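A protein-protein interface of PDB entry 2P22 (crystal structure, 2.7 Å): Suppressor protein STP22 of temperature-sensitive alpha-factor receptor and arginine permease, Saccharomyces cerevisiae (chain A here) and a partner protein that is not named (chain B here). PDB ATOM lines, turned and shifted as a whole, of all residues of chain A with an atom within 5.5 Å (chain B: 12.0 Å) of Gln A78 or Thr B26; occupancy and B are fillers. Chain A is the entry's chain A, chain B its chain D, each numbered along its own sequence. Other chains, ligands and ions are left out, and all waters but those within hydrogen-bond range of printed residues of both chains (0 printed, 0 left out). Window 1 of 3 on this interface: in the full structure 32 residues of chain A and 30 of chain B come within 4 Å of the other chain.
Ser A74 touches Phe B28. Leu A75 touches Phe B28. Gln A78 touches Val B25. Gln A78 touches Thr B26 (OE1 to O, 3.6 Å). Phe B28 touches Gln A78. CG1 of Val B25 touches CD1 of Leu A82 (3.5 Å).
Ser A74 touches one residue of chain B. No residue of chain B comes within 4 Å of Asn A76. Gln A78 touches three residues of chain B. No residue of chain B comes within 4 Å of Ile A79. No residue of chain B comes within 4 Å of Asp A80. Val A81 touches none of the printed residues of chain B. Thr B24 touches none of the printed residues of chain A. Printed residues of chain A within 4 Å of Val B25: Gln A78 and Leu A82. Printed residues of chain A within 4 Å of Thr B26: Gln A78 (3.6 Å). Of the printed residues of chain A, Phe B28 touches Ser A74 (3.6 Å), Leu A75 (3.5 Å) and Gln A78 (3.95 Å). The nearest printed residue of chain A that does not touch Thr B26 is Leu A82 (6.1 Å). The nearest printed residue of chain A that does not touch Phe B28 is His A73 (7.0 Å).
Of the 10 printed residues of chain A, 4 touch a printed residue of chain B. Hydrophobic or aromatic side chains of chain B that line the printed part of chain A: Val B25 and Phe B28. Among the printed residues, no Asp or Glu carboxylate lies within 4 Å of a Lys or Arg side-chain nitrogen of the other chain.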
ATOM      1  N   HIS A  73      32.877 -34.961  32.669  1.00  0.00           N
ATOM      2  CA  HIS A  73      32.264 -34.237  33.776  1.00  0.00           C
ATOM      3  C   HIS A  73      32.042 -32.781  33.358  1.00  0.00           C
ATOM      4  O   HIS A  73      31.139 -32.111  33.856  1.00  0.00           O
ATOM      5  CB  HIS A  73      33.151 -34.301  35.030  1.00  0.00           C
ATOM      6  CG  HIS A  73      32.380 -34.257  36.318  1.00  0.00           C
ATOM      7  ND1 HIS A  73      31.557 -35.285  36.730  1.00  0.00           N
ATOM      8  CD2 HIS A  73      32.284 -33.297  37.269  1.00  0.00           C
ATOM      9  CE1 HIS A  73      30.985 -34.959  37.877  1.00  0.00           C
ATOM     10  NE2 HIS A  73      31.409 -33.756  38.225  1.00  0.00           N
ATOM     11  N   SER A  74      32.861 -32.299  32.431  1.00  0.00           N
ATOM     12  CA  SER A  74      32.729 -30.932  31.954  1.00  0.00           C
ATOM     13  C   SER A  74      31.493 -30.809  31.085  1.00  0.00           C
ATOM     14  O   SER A  74      30.842 -29.766  31.046  1.00  0.00           O
ATOM     15  CB  SER A  74      33.959 -30.524  31.146  1.00  0.00           C
ATOM     16  OG  SER A  74      35.103 -30.463  31.974  1.00  0.00           O
ATOM     17  N   LEU A  75      31.170 -31.883  30.385  1.00  0.00           N
ATOM     18  CA  LEU A  75      30.008 -31.876  29.522  1.00  0.00           C
ATOM     19  C   LEU A  75      28.723 -31.985  30.327  1.00  0.00           C
ATOM     20  O   LEU A  75      27.811 -31.180  30.153  1.00  0.00           O
ATOM     21  CB  LEU A  75      30.093 -33.022  28.521  1.00  0.00           C
ATOM     22  CG  LEU A  75      31.266 -32.932  27.547  1.00  0.00           C
ATOM     23  CD1 LEU A  75      31.309 -34.202  26.724  1.00  0.00           C
ATOM     24  CD2 LEU A  75      31.130 -31.706  26.655  1.00  0.00           C
ATOM     25  N   ASN A  76      28.648 -32.971  31.217  1.00  0.00           N
ATOM     26  CA  ASN A  76      27.440 -33.146  32.011  1.00  0.00           C
ATOM     27  C   ASN A  76      27.229 -31.969  32.957  1.00  0.00           C
ATOM     28  O   ASN A  76      26.204 -31.876  33.635  1.00  0.00           O
ATOM     29  CB  ASN A  76      27.485 -34.461  32.798  1.00  0.00           C
ATOM     30  CG  ASN A  76      28.601 -34.494  33.818  1.00  0.00           C
ATOM     31  OD1 ASN A  76      28.687 -33.631  34.697  1.00  0.00           O
ATOM     32  ND2 ASN A  76      29.464 -35.498  33.713  1.00  0.00           N
ATOM     33  N   ALA A  77      28.201 -31.066  32.991  1.00  0.00           N
ATOM     34  CA  ALA A  77      28.119 -29.893  33.841  1.00  0.00           C
ATOM     35  C   ALA A  77      27.813 -28.690  32.969  1.00  0.00           C
ATOM     36  O   ALA A  77      27.031 -27.820  33.342  1.00  0.00           O
ATOM     37  CB  ALA A  77      29.434 -29.685  34.574  1.00  0.00           C
ATOM     38  N   GLN A  78      28.436 -28.651  31.797  1.00  0.00           N
ATOM     39  CA  GLN A  78      28.236 -27.551  30.864  1.00  0.00           C
ATOM     40  C   GLN A  78      26.825 -27.600  30.298  1.00  0.00           C
ATOM     41  O   GLN A  78      26.352 -26.620  29.729  1.00  0.00           O
ATOM     42  CB  GLN A  78      29.245 -27.637  29.721  1.00  0.00           C
ATOM     43  CG  GLN A  78      29.260 -26.418  28.824  1.00  0.00           C
ATOM     44  CD  GLN A  78      29.894 -25.221  29.492  1.00  0.00           C
ATOM     45  OE1 GLN A  78      29.907 -24.122  28.938  1.00  0.00           O
ATOM     46  NE2 GLN A  78      30.432 -25.428  30.689  1.00  0.00           N
ATOM     47  N   ILE A  79      26.158 -28.741  30.454  1.00  0.00           N
ATOM     48  CA  ILE A  79      24.795 -28.892  29.951  1.00  0.00           C
ATOM     49  C   ILE A  79      23.763 -28.387  30.953  1.00  0.00           C
ATOM     50  O   ILE A  79      22.671 -27.967  30.566  1.00  0.00           O
ATOM     51  CB  ILE A  79      24.447 -30.359  29.625  1.00  0.00           C
ATOM     52  CG1 ILE A  79      24.586 -31.210  30.883  1.00  0.00           C
ATOM     53  CG2 ILE A  79      25.330 -30.880  28.500  1.00  0.00           C
ATOM     54  CD1 ILE A  79      23.983 -32.595  30.756  1.00  0.00           C
ATOM     55  N   ASP A  80      24.098 -28.434  32.241  1.00  0.00           N
ATOM     56  CA  ASP A  80      23.166 -27.968  33.265  1.00  0.00           C
ATOM     57  C   ASP A  80      23.065 -26.443  33.233  1.00  0.00           C
ATOM     58  O   ASP A  80      21.987 -25.880  33.417  1.00  0.00           O
ATOM     59  CB  ASP A  80      23.606 -28.429  34.664  1.00  0.00           C
ATOM     60  CG  ASP A  80      23.738 -29.939  34.772  1.00  0.00           C
ATOM     61  OD1 ASP A  80      22.828 -30.667  34.320  1.00  0.00           O
ATOM     62  OD2 ASP A  80      24.755 -30.401  35.323  1.00  0.00           O
ATOM     63  N   VAL A  81      24.196 -25.784  32.996  1.00  0.00           N
ATOM     64  CA  VAL A  81      24.236 -24.329  32.928  1.00  0.00           C
ATOM     65  C   VAL A  81      23.671 -23.869  31.593  1.00  0.00           C
ATOM     66  O   VAL A  81      23.510 -22.676  31.346  1.00  0.00           O
ATOM     67  CB  VAL A  81      25.676 -23.799  33.050  1.00  0.00           C
ATOM     68  CG1 VAL A  81      26.308 -24.305  34.339  1.00  0.00           C
ATOM     69  CG2 VAL A  81      26.489 -24.231  31.844  1.00  0.00           C
ATOM     70  N   LEU A  82      23.382 -24.834  30.731  1.00  0.00           N
ATOM     71  CA  LEU A  82      22.835 -24.541  29.422  1.00  0.00           C
ATOM     72  C   LEU A  82      21.322 -24.735  29.488  1.00  0.00           C
ATOM     73  O   LEU A  82      20.563 -23.862  29.079  1.00  0.00           O
ATOM     74  CB  LEU A  82      23.464 -25.470  28.375  1.00  0.00           C
ATOM     75  CG  LEU A  82      23.738 -24.864  26.991  1.00  0.00           C
ATOM     76  CD1 LEU A  82      24.538 -23.582  27.152  1.00  0.00           C
ATOM     77  CD2 LEU A  82      24.495 -25.841  26.119  1.00  0.00           C
ATOM     78  N   GLN B  22      21.590 -12.589  27.482  1.00  0.00           N
ATOM     79  CA  GLN B  22      22.887 -12.471  26.815  1.00  0.00           C
ATOM     80  C   GLN B  22      23.631 -13.812  26.836  1.00  0.00           C
ATOM     81  O   GLN B  22      23.416 -14.641  27.725  1.00  0.00           O
ATOM     82  CB  GLN B  22      23.752 -11.411  27.510  1.00  0.00           C
ATOM     83  CG  GLN B  22      23.049 -10.093  27.787  1.00  0.00           C
ATOM     84  CD  GLN B  22      22.598  -9.380  26.524  1.00  0.00           C
ATOM     85  OE1 GLN B  22      21.774  -8.467  26.584  1.00  0.00           O
ATOM     86  NE2 GLN B  22      23.140  -9.786  25.378  1.00  0.00           N
ATOM     87  N   GLU B  23      24.511 -14.009  25.854  1.00  0.00           N
ATOM     88  CA  GLU B  23      25.309 -15.228  25.748  1.00  0.00           C
ATOM     89  C   GLU B  23      26.399 -15.292  26.813  1.00  0.00           C
ATOM     90  O   GLU B  23      27.558 -14.977  26.550  1.00  0.00           O
ATOM     91  CB  GLU B  23      25.953 -15.326  24.364  1.00  0.00           C
ATOM     92  CG  GLU B  23      25.000 -15.732  23.257  1.00  0.00           C
ATOM     93  CD  GLU B  23      25.701 -15.942  21.916  1.00  0.00           C
ATOM     94  OE1 GLU B  23      26.681 -16.717  21.867  1.00  0.00           O
ATOM     95  OE2 GLU B  23      25.269 -15.336  20.913  1.00  0.00           O
ATOM     96  N   THR B  24      26.022 -15.704  28.016  1.00  0.00           N
ATOM     97  CA  THR B  24      26.972 -15.814  29.113  1.00  0.00           C
ATOM     98  C   THR B  24      27.680 -17.166  29.059  1.00  0.00           C
ATOM     99  O   THR B  24      28.574 -17.440  29.857  1.00  0.00           O
ATOM    100  CB  THR B  24      26.263 -15.666  30.487  1.00  0.00           C
ATOM    101  OG1 THR B  24      25.183 -16.605  30.582  1.00  0.00           O
ATOM    102  CG2 THR B  24      25.722 -14.263  30.653  1.00  0.00           C
ATOM    103  N   VAL B  25      27.271 -18.011  28.115  1.00  0.00           N
ATOM    104  CA  VAL B  25      27.862 -19.338  27.958  1.00  0.00           C
ATOM    105  C   VAL B  25      28.643 -19.435  26.650  1.00  0.00           C
ATOM    106  O   VAL B  25      28.152 -19.048  25.588  1.00  0.00           O
ATOM    107  CB  VAL B  25      26.781 -20.437  27.956  1.00  0.00           C
ATOM    108  CG1 VAL B  25      27.425 -21.816  27.999  1.00  0.00           C
ATOM    109  CG2 VAL B  25      25.938 -20.285  29.103  1.00  0.00           C
ATOM    110  N   THR B  26      29.861 -19.956  26.728  1.00  0.00           N
ATOM    111  CA  THR B  26      30.688 -20.094  25.538  1.00  0.00           C
ATOM    112  C   THR B  26      30.649 -21.530  25.044  1.00  0.00           C
ATOM    113  O   THR B  26      30.396 -22.459  25.816  1.00  0.00           O
ATOM    114  CB  THR B  26      32.145 -19.714  25.821  1.00  0.00           C
ATOM    115  OG1 THR B  26      32.180 -18.582  26.697  1.00  0.00           O
ATOM    116  CG2 THR B  26      32.854 -19.358  24.522  1.00  0.00           C
ATOM    117  N   ARG B  27      30.899 -21.712  23.752  1.00  0.00           N
ATOM    118  CA  ARG B  27      30.885 -23.046  23.179  1.00  0.00           C
ATOM    119  C   ARG B  27      32.055 -23.848  23.714  1.00  0.00           C
ATOM    120  O   ARG B  27      33.210 -23.481  23.512  1.00  0.00           O
ATOM    121  CB  ARG B  27      30.970 -22.986  21.655  1.00  0.00           C
ATOM    122  CG  ARG B  27      30.681 -24.324  20.999  1.00  0.00           C
ATOM    123  CD  ARG B  27      30.968 -24.309  19.503  1.00  0.00           C
ATOM    124  NE  ARG B  27      30.602 -25.571  18.856  1.00  0.00           N
ATOM    125  CZ  ARG B  27      31.045 -26.772  19.226  1.00  0.00           C
ATOM    126  NH1 ARG B  27      31.879 -26.893  20.251  1.00  0.00           N
ATOM    127  NH2 ARG B  27      30.660 -27.856  18.566  1.00  0.00           N
ATOM    128  N   PHE B  28      31.745 -24.940  24.409  1.00  0.00           N
ATOM    129  CA  PHE B  28      32.765 -25.819  24.976  1.00  0.00           C
ATOM    130  C   PHE B  28      33.190 -26.824  23.918  1.00  0.00           C
ATOM    131  O   PHE B  28      32.478 -27.789  23.655  1.00  0.00           O
ATOM    132  CB  PHE B  28      32.207 -26.561  26.193  1.00  0.00           C
ATOM    133  CG  PHE B  28      33.148 -27.590  26.771  1.00  0.00           C
ATOM    134  CD1 PHE B  28      33.206 -28.884  26.251  1.00  0.00           C
ATOM    135  CD2 PHE B  28      33.973 -27.264  27.844  1.00  0.00           C
ATOM    136  CE1 PHE B  28      34.073 -29.835  26.793  1.00  0.00           C
ATOM    137  CE2 PHE B  28      34.844 -28.209  28.393  1.00  0.00           C
ATOM    138  CZ  PHE B  28      34.892 -29.495  27.867  1.00  0.00           C
ATOM    139  N   GLN B  29      34.349 -26.599  23.312  1.00  0.00           N
ATOM    140  CA  GLN B  29      34.839 -27.500  22.276  1.00  0.00           C
ATOM    141  C   GLN B  29      35.556 -28.720  22.842  1.00  0.00           C
ATOM    142  O   GLN B  29      36.513 -28.596  23.602  1.00  0.00           O
ATOM    143  CB  GLN B  29      35.775 -26.754  21.338  1.00  0.00           C
ATOM    144  CG  GLN B  29      36.930 -26.111  22.046  1.00  0.00           C
ATOM    145  CD  GLN B  29      37.876 -25.461  21.077  1.00  0.00           C
ATOM    146  OE1 GLN B  29      38.497 -26.137  20.255  1.00  0.00           O
ATOM    147  NE2 GLN B  29      37.991 -24.141  21.157  1.00  0.00           N
ATOM    148  N   MET B  30      35.078 -29.898  22.452  1.00  0.00           N
ATOM    149  CA  MET B  30      35.651 -31.157  22.903  1.00  0.00           C
ATOM    150  C   MET B  30      37.061 -31.342  22.348  1.00  0.00           C
ATOM    151  O   MET B  30      37.344 -31.005  21.201  1.00  0.00           O
ATOM    152  CB  MET B  30      34.759 -32.326  22.461  1.00  0.00           C
ATOM    153  CG  MET B  30      35.224 -33.708  22.942  1.00  0.00           C
ATOM    154  SD  MET B  30      34.160 -35.087  22.401  1.00  0.00           S
ATOM    155  CE  MET B  30      35.028 -35.646  20.907  1.00  0.00           C
ATOM    156  N   PRO B  31      37.976 -31.864  23.173  1.00  0.00           N
ATOM    157  CA  PRO B  31      39.349 -32.083  22.731  1.00  0.00           C
ATOM    158  C   PRO B  31      39.449 -33.318  21.829  1.00  0.00           C
ATOM    159  O   PRO B  31      38.497 -34.094  21.703  1.00  0.00           O
ATOM    160  CB  PRO B  31      40.100 -32.258  24.046  1.00  0.00           C
ATOM    161  CG  PRO B  31      39.093 -32.948  24.901  1.00  0.00           C
ATOM    162  CD  PRO B  31      37.837 -32.159  24.610  1.00  0.00           C
